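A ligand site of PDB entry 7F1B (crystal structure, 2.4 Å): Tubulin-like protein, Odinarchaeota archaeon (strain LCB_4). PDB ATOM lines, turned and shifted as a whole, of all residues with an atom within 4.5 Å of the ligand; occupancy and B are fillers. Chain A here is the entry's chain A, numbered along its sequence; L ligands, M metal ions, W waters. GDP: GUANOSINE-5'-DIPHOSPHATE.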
ATOM      1  N   GLY A  12      20.827 -19.363   6.059  1.00  0.00           N
ATOM      2  CA  GLY A  12      20.153 -19.869   4.884  1.00  0.00           C
ATOM      3  C   GLY A  12      20.330 -18.958   3.677  1.00  0.00           C
ATOM      4  O   GLY A  12      20.811 -17.824   3.768  1.00  0.00           O
ATOM      5  N   GLN A  13      19.906 -19.482   2.530  1.00  0.00           N
ATOM      6  CA  GLN A  13      20.092 -18.761   1.277  1.00  0.00           C
ATOM      7  C   GLN A  13      19.324 -17.442   1.272  1.00  0.00           C
ATOM      8  O   GLN A  13      19.886 -16.389   0.988  1.00  0.00           O
ATOM      9  CB  GLN A  13      19.670 -19.636   0.091  1.00  0.00           C
ATOM     10  CG  GLN A  13      19.840 -18.963  -1.257  1.00  0.00           C
ATOM     11  CD  GLN A  13      19.714 -19.922  -2.416  1.00  0.00           C
ATOM     12  OE1 GLN A  13      19.290 -21.065  -2.250  1.00  0.00           O
ATOM     13  NE2 GLN A  13      20.095 -19.472  -3.611  1.00  0.00           N
ATOM     14  N   GLY A  14      18.034 -17.499   1.587  1.00  0.00           N
ATOM     15  CA  GLY A  14      17.228 -16.283   1.587  1.00  0.00           C
ATOM     16  C   GLY A  14      17.732 -15.254   2.586  1.00  0.00           C
ATOM     17  O   GLY A  14      17.759 -14.060   2.293  1.00  0.00           O
ATOM     18  N   GLN A  17      20.994 -13.626   1.107  1.00  0.00           N
ATOM     19  CA  GLN A  17      20.723 -12.769  -0.030  1.00  0.00           C
ATOM     20  C   GLN A  17      20.019 -11.476   0.385  1.00  0.00           C
ATOM     21  O   GLN A  17      20.252 -10.426  -0.212  1.00  0.00           O
ATOM     22  CB  GLN A  17      19.889 -13.515  -1.077  1.00  0.00           C
ATOM     23  CG  GLN A  17      20.633 -14.653  -1.740  1.00  0.00           C
ATOM     24  CD  GLN A  17      19.743 -15.489  -2.651  1.00  0.00           C
ATOM     25  OE1 GLN A  17      18.519 -15.335  -2.641  1.00  0.00           O
ATOM     26  NE2 GLN A  17      20.346 -16.359  -3.441  1.00  0.00           N
ATOM     27  N   ASP A  69      25.546 -20.629   6.388  1.00  0.00           N
ATOM     28  CA  ASP A  69      24.796 -21.353   5.381  1.00  0.00           C
ATOM     29  C   ASP A  69      25.358 -22.757   5.248  1.00  0.00           C
ATOM     30  O   ASP A  69      26.537 -23.002   5.535  1.00  0.00           O
ATOM     31  CB  ASP A  69      24.814 -20.629   4.031  1.00  0.00           C
ATOM     32  CG  ASP A  69      23.602 -20.943   3.185  1.00  0.00           C
ATOM     33  OD1 ASP A  69      22.955 -21.987   3.426  1.00  0.00           O
ATOM     34  OD2 ASP A  69      23.286 -20.139   2.288  1.00  0.00           O
ATOM     35  N   ASN A 102      15.738 -28.376   1.875  1.00  0.00           N
ATOM     36  CA  ASN A 102      14.438 -27.785   2.222  1.00  0.00           C
ATOM     37  C   ASN A 102      13.729 -28.558   3.322  1.00  0.00           C
ATOM     38  O   ASN A 102      12.499 -28.617   3.351  1.00  0.00           O
ATOM     39  CB  ASN A 102      13.540 -27.656   0.996  1.00  0.00           C
ATOM     40  CG  ASN A 102      13.426 -26.236   0.491  1.00  0.00           C
ATOM     41  OD1 ASN A 102      12.477 -25.514   0.829  1.00  0.00           O
ATOM     42  ND2 ASN A 102      14.380 -25.812  -0.322  1.00  0.00           N
ATOM     43  N   THR A 138      14.663 -17.186   6.518  1.00  0.00           N
ATOM     44  CA  THR A 138      13.342 -17.602   6.063  1.00  0.00           C
ATOM     45  C   THR A 138      12.892 -18.830   6.853  1.00  0.00           C
ATOM     46  O   THR A 138      13.681 -19.514   7.497  1.00  0.00           O
ATOM     47  CB  THR A 138      13.338 -17.916   4.568  1.00  0.00           C
ATOM     48  OG1 THR A 138      14.100 -19.111   4.327  1.00  0.00           O
ATOM     49  CG2 THR A 138      13.963 -16.768   3.782  1.00  0.00           C
ATOM     50  N   GLY A 140      10.496 -21.170   5.331  1.00  0.00           N
ATOM     51  CA  GLY A 140       9.945 -22.180   4.441  1.00  0.00           C
ATOM     52  C   GLY A 140      10.915 -23.260   4.015  1.00  0.00           C
ATOM     53  O   GLY A 140      10.484 -24.370   3.669  1.00  0.00           O
ATOM     54  N   GLY A 141      12.203 -22.973   4.038  1.00  0.00           N
ATOM     55  CA  GLY A 141      13.229 -23.890   3.588  1.00  0.00           C
ATOM     56  C   GLY A 141      13.712 -24.813   4.688  1.00  0.00           C
ATOM     57  O   GLY A 141      12.986 -25.138   5.623  1.00  0.00           O
ATOM     58  N   GLY A 142      14.961 -25.248   4.553  1.00  0.00           N
ATOM     59  CA  GLY A 142      15.550 -26.168   5.508  1.00  0.00           C
ATOM     60  C   GLY A 142      16.632 -25.563   6.378  1.00  0.00           C
ATOM     61  O   GLY A 142      16.654 -25.782   7.592  1.00  0.00           O
ATOM     62  N   THR A 143      17.527 -24.782   5.769  1.00  0.00           N
ATOM     63  CA  THR A 143      18.620 -24.185   6.532  1.00  0.00           C
ATOM     64  C   THR A 143      18.127 -23.047   7.407  1.00  0.00           C
ATOM     65  O   THR A 143      18.223 -23.106   8.645  1.00  0.00           O
ATOM     66  CB  THR A 143      19.720 -23.699   5.587  1.00  0.00           C
ATOM     67  OG1 THR A 143      20.214 -24.809   4.813  1.00  0.00           O
ATOM     68  CG2 THR A 143      20.879 -23.109   6.375  1.00  0.00           C
ATOM     69  N   GLY A 144      17.574 -21.996   6.794  1.00  0.00           N
ATOM     70  CA  GLY A 144      17.079 -20.878   7.575  1.00  0.00           C
ATOM     71  C   GLY A 144      16.026 -21.275   8.587  1.00  0.00           C
ATOM     72  O   GLY A 144      15.940 -20.674   9.663  1.00  0.00           O
ATOM     73  N   VAL A 169      11.060 -14.685   7.501  1.00  0.00           N
ATOM     74  CA  VAL A 169      10.306 -14.559   6.269  1.00  0.00           C
ATOM     75  C   VAL A 169       9.397 -15.774   6.116  1.00  0.00           C
ATOM     76  O   VAL A 169       9.867 -16.922   6.147  1.00  0.00           O
ATOM     77  CB  VAL A 169      11.233 -14.410   5.049  1.00  0.00           C
ATOM     78  CG1 VAL A 169      10.420 -14.183   3.782  1.00  0.00           C
ATOM     79  CG2 VAL A 169      12.226 -13.272   5.271  1.00  0.00           C
ATOM     80  N   PRO A 171       6.712 -18.237   4.003  1.00  0.00           N
ATOM     81  CA  PRO A 171       6.605 -18.673   2.602  1.00  0.00           C
ATOM     82  C   PRO A 171       5.398 -18.045   1.914  1.00  0.00           C
ATOM     83  O   PRO A 171       4.516 -17.456   2.539  1.00  0.00           O
ATOM     84  CB  PRO A 171       6.443 -20.195   2.711  1.00  0.00           C
ATOM     85  CG  PRO A 171       6.862 -20.541   4.102  1.00  0.00           C
ATOM     86  CD  PRO A 171       6.544 -19.356   4.949  1.00  0.00           C
ATOM     87  N   SER A 172       5.383 -18.195   0.594  1.00  0.00           N
ATOM     88  CA  SER A 172       4.208 -17.801  -0.181  1.00  0.00           C
ATOM     89  C   SER A 172       3.063 -18.773   0.083  1.00  0.00           C
ATOM     90  O   SER A 172       3.257 -19.994   0.080  1.00  0.00           O
ATOM     91  CB  SER A 172       4.548 -17.770  -1.677  1.00  0.00           C
ATOM     92  OG  SER A 172       3.373 -17.660  -2.459  1.00  0.00           O
ATOM     93  N   ASP A 176       4.451 -21.877  -3.335  1.00  0.00           N
ATOM     94  CA  ASP A 176       5.659 -22.265  -2.622  1.00  0.00           C
ATOM     95  C   ASP A 176       5.753 -23.793  -2.585  1.00  0.00           C
ATOM     96  O   ASP A 176       4.824 -24.499  -2.981  1.00  0.00           O
ATOM     97  CB  ASP A 176       5.695 -21.682  -1.204  1.00  0.00           C
ATOM     98  CG  ASP A 176       7.103 -21.334  -0.763  1.00  0.00           C
ATOM     99  OD1 ASP A 176       7.992 -22.203  -0.877  1.00  0.00           O
ATOM    100  OD2 ASP A 176       7.317 -20.183  -0.323  1.00  0.00           O
ATOM    101  N   ASN A 203       6.192 -13.334   1.895  1.00  0.00           N
ATOM    102  CA  ASN A 203       6.372 -13.143   0.457  1.00  0.00           C
ATOM    103  C   ASN A 203       5.041 -12.940  -0.254  1.00  0.00           C
ATOM    104  O   ASN A 203       4.996 -12.298  -1.318  1.00  0.00           O
ATOM    105  CB  ASN A 203       7.119 -14.334  -0.151  1.00  0.00           C
ATOM    106  CG  ASN A 203       8.597 -14.309   0.154  1.00  0.00           C
ATOM    107  OD1 ASN A 203       9.214 -13.254   0.232  1.00  0.00           O
ATOM    108  ND2 ASN A 203       9.185 -15.494   0.330  1.00  0.00           N
ATOM    109  N   LEU A 225      12.642  -9.004  -4.649  1.00  0.00           N
ATOM    110  CA  LEU A 225      11.864  -9.197  -3.434  1.00  0.00           C
ATOM    111  C   LEU A 225      12.730  -9.068  -2.190  1.00  0.00           C
ATOM    112  O   LEU A 225      12.466  -8.247  -1.308  1.00  0.00           O
ATOM    113  CB  LEU A 225      11.161 -10.561  -3.467  1.00  0.00           C
ATOM    114  CG  LEU A 225       9.699 -10.576  -3.912  1.00  0.00           C
ATOM    115  CD1 LEU A 225       9.066 -11.937  -3.670  1.00  0.00           C
ATOM    116  CD2 LEU A 225       8.911  -9.485  -3.201  1.00  0.00           C
ATOM    117  N   ASN A 226      13.797  -9.879  -2.112  1.00  0.00           N
ATOM    118  CA  ASN A 226      14.706  -9.791  -0.983  1.00  0.00           C
ATOM    119  C   ASN A 226      15.368  -8.421  -0.900  1.00  0.00           C
ATOM    120  O   ASN A 226      15.727  -7.964   0.184  1.00  0.00           O
ATOM    121  CB  ASN A 226      15.777 -10.883  -1.060  1.00  0.00           C
ATOM    122  CG  ASN A 226      16.511 -10.882  -2.380  1.00  0.00           C
ATOM    123  OD1 ASN A 226      16.189 -11.646  -3.286  1.00  0.00           O
ATOM    124  ND2 ASN A 226      17.516 -10.008  -2.503  1.00  0.00           N
ATOM    125  N   ILE A 229      12.781  -6.476   0.877  1.00  0.00           N
ATOM    126  CA  ILE A 229      12.704  -6.900   2.272  1.00  0.00           C
ATOM    127  C   ILE A 229      13.836  -6.275   3.080  1.00  0.00           C
ATOM    128  O   ILE A 229      13.635  -5.867   4.237  1.00  0.00           O
ATOM    129  CB  ILE A 229      12.726  -8.439   2.378  1.00  0.00           C
ATOM    130  CG1 ILE A 229      11.539  -9.047   1.622  1.00  0.00           C
ATOM    131  CG2 ILE A 229      12.684  -8.867   3.837  1.00  0.00           C
ATOM    132  CD1 ILE A 229      11.116 -10.401   2.125  1.00  0.00           C
HETATM  133  PB  GDP L   1      17.323 -22.546   2.974  1.00  0.00           P
HETATM  134  O1B GDP L   1      17.011 -23.908   3.532  1.00  0.00           O
HETATM  135  O2B GDP L   1      18.781 -22.503   2.579  1.00  0.00           O
HETATM  136  O3B GDP L   1      17.034 -21.498   4.024  1.00  0.00           O
HETATM  137  O3A GDP L   1      16.417 -22.328   1.655  1.00  0.00           O
HETATM  138  PA  GDP L   1      15.624 -20.956   1.334  1.00  0.00           P
HETATM  139  O1A GDP L   1      16.130 -19.795   2.151  1.00  0.00           O
HETATM  140  O2A GDP L   1      15.736 -20.639  -0.137  1.00  0.00           O
HETATM  141  O5' GDP L   1      14.106 -21.320   1.701  1.00  0.00           O
HETATM  142  C5' GDP L   1      13.107 -21.300   0.687  1.00  0.00           C
HETATM  143  C4' GDP L   1      11.934 -20.457   1.151  1.00  0.00           C
HETATM  144  O4' GDP L   1      12.438 -19.173   1.535  1.00  0.00           O
HETATM  145  C3' GDP L   1      10.944 -20.259   0.023  1.00  0.00           C
HETATM  146  O3' GDP L   1       9.653 -20.694   0.459  1.00  0.00           O
HETATM  147  C2' GDP L   1      10.931 -18.771  -0.274  1.00  0.00           C
HETATM  148  O2' GDP L   1       9.605 -18.266  -0.128  1.00  0.00           O
HETATM  149  C1' GDP L   1      11.861 -18.133   0.744  1.00  0.00           C
HETATM  150  N9  GDP L   1      12.969 -17.396   0.088  1.00  0.00           N
HETATM  151  C8  GDP L   1      14.097 -17.954  -0.401  1.00  0.00           C
HETATM  152  N7  GDP L   1      14.922 -17.020  -0.927  1.00  0.00           N
HETATM  153  C5  GDP L   1      14.318 -15.827  -0.779  1.00  0.00           C
HETATM  154  C6  GDP L   1      14.644 -14.428  -1.129  1.00  0.00           C
HETATM  155  O6  GDP L   1      15.716 -14.127  -1.694  1.00  0.00           O
HETATM  156  N1  GDP L   1      13.750 -13.476  -0.812  1.00  0.00           N
HETATM  157  C2  GDP L   1      12.582 -13.768  -0.189  1.00  0.00           C
HETATM  158  N2  GDP L   1      11.733 -12.755   0.094  1.00  0.00           N
HETATM  159  N3  GDP L   1      12.228 -15.034   0.151  1.00  0.00           N
HETATM  160  C4  GDP L   1      13.037 -16.077  -0.117  1.00  0.00           C
HETATM  161 MG    MG M   1      17.413 -23.776  -1.816  1.00  0.00          MG
HETATM  162  O   HOH W   1      18.739 -23.174  -0.427  1.00  0.00           O
HETATM  163  O   HOH W   2      17.707 -26.062   1.817  1.00  0.00           O
HETATM  164  O   HOH W   3      14.468 -21.744   5.574  1.00  0.00           O
HETATM  165  O   HOH W   4      17.166 -18.319   4.931  1.00  0.00           O
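The side-chain amide oxygen (OD1) of Asn 226 sits close to an oxygen (O6) of the ligand (3.0 Å). The backbone NH of Gln 13 lies within hydrogen-bond range of an oxygen (O2B) of the ligand (3.2 Å). OE1 of Gln 17 sits close to O6 of the ligand, 3.2 Å away. O5' of the ligand lies close to N of Gly 141 (3.4 Å). O1A of the ligand is in hydrogen-bond range of OG1 of Thr 138 (3.1 Å). An oxygen (O1B) of the ligand lies within hydrogen-bond range of the backbone NH (N) of Gly 142 (2.7 Å). O1B of the ligand is in hydrogen-bond range of N of Thr 143, 2.5 Å away. The backbone NH of Gly 14 is in hydrogen-bond range of an oxygen (O1A) of the ligand (3.0 Å). The side-chain carboxylate (OD2) of Asp 176 is in hydrogen-bond range of an oxygen (O3') of the ligand (2.5 Å). N of Gly 144 lies within hydrogen-bond range of O3B of the ligand, 2.9 Å away. The side-chain amide oxygen (OD1) of Asn 203 lies within hydrogen-bond range of a nitrogen (N2) of the ligand (2.6 Å).
N of Gln 13 lies within hydrogen-bond range of OD2 of Asp 69, at 3.5 Å. The side-chain amide nitrogen of Gln 13 sits close to the side-chain amide nitrogen of Gln 17 (3.1 Å). OD2 of Asp 176 is in hydrogen-bond range of N of Ser 172, 2.9 Å away.
Gly 12 touches the ligand. Pro 171 touches the ligand. Ile 229 touches the ligand. Hydrophobic or aromatic side chains within 4 Å of the ligand: Pro 171 and Ile 229. 14 residues have an atom within 4 Å of the ligand: Gly 12, Gln 13, Gly 14, Gln 17, Thr 138, Gly 141, Gly 142, Thr 143, Gly 144, Pro 171, Asp 176, Asn 203, Asn 226 and Ile 229. Along chain A the residues within 4 Å of the ligand span positions 12 to 229.
Water W2 bridges O1B of the ligand (2.8 Å) and N of Asn 102 (3.0 Å). Water W3 lies within hydrogen-bond range of OG1 of Thr 138 (2.9 Å), N of Gly 141 (3.0 Å), O3B of the ligand (3.0 Å) and N of Gly 144 (3.3 Å). Water W1 bridges OE1 of Gln 13 (2.8 Å) and O2B of the ligand (3.1 Å). Water W4 bridges the backbone NH (N) of Thr 138 (3.2 Å) and an oxygen (O3B) of the ligand (3.3 Å).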
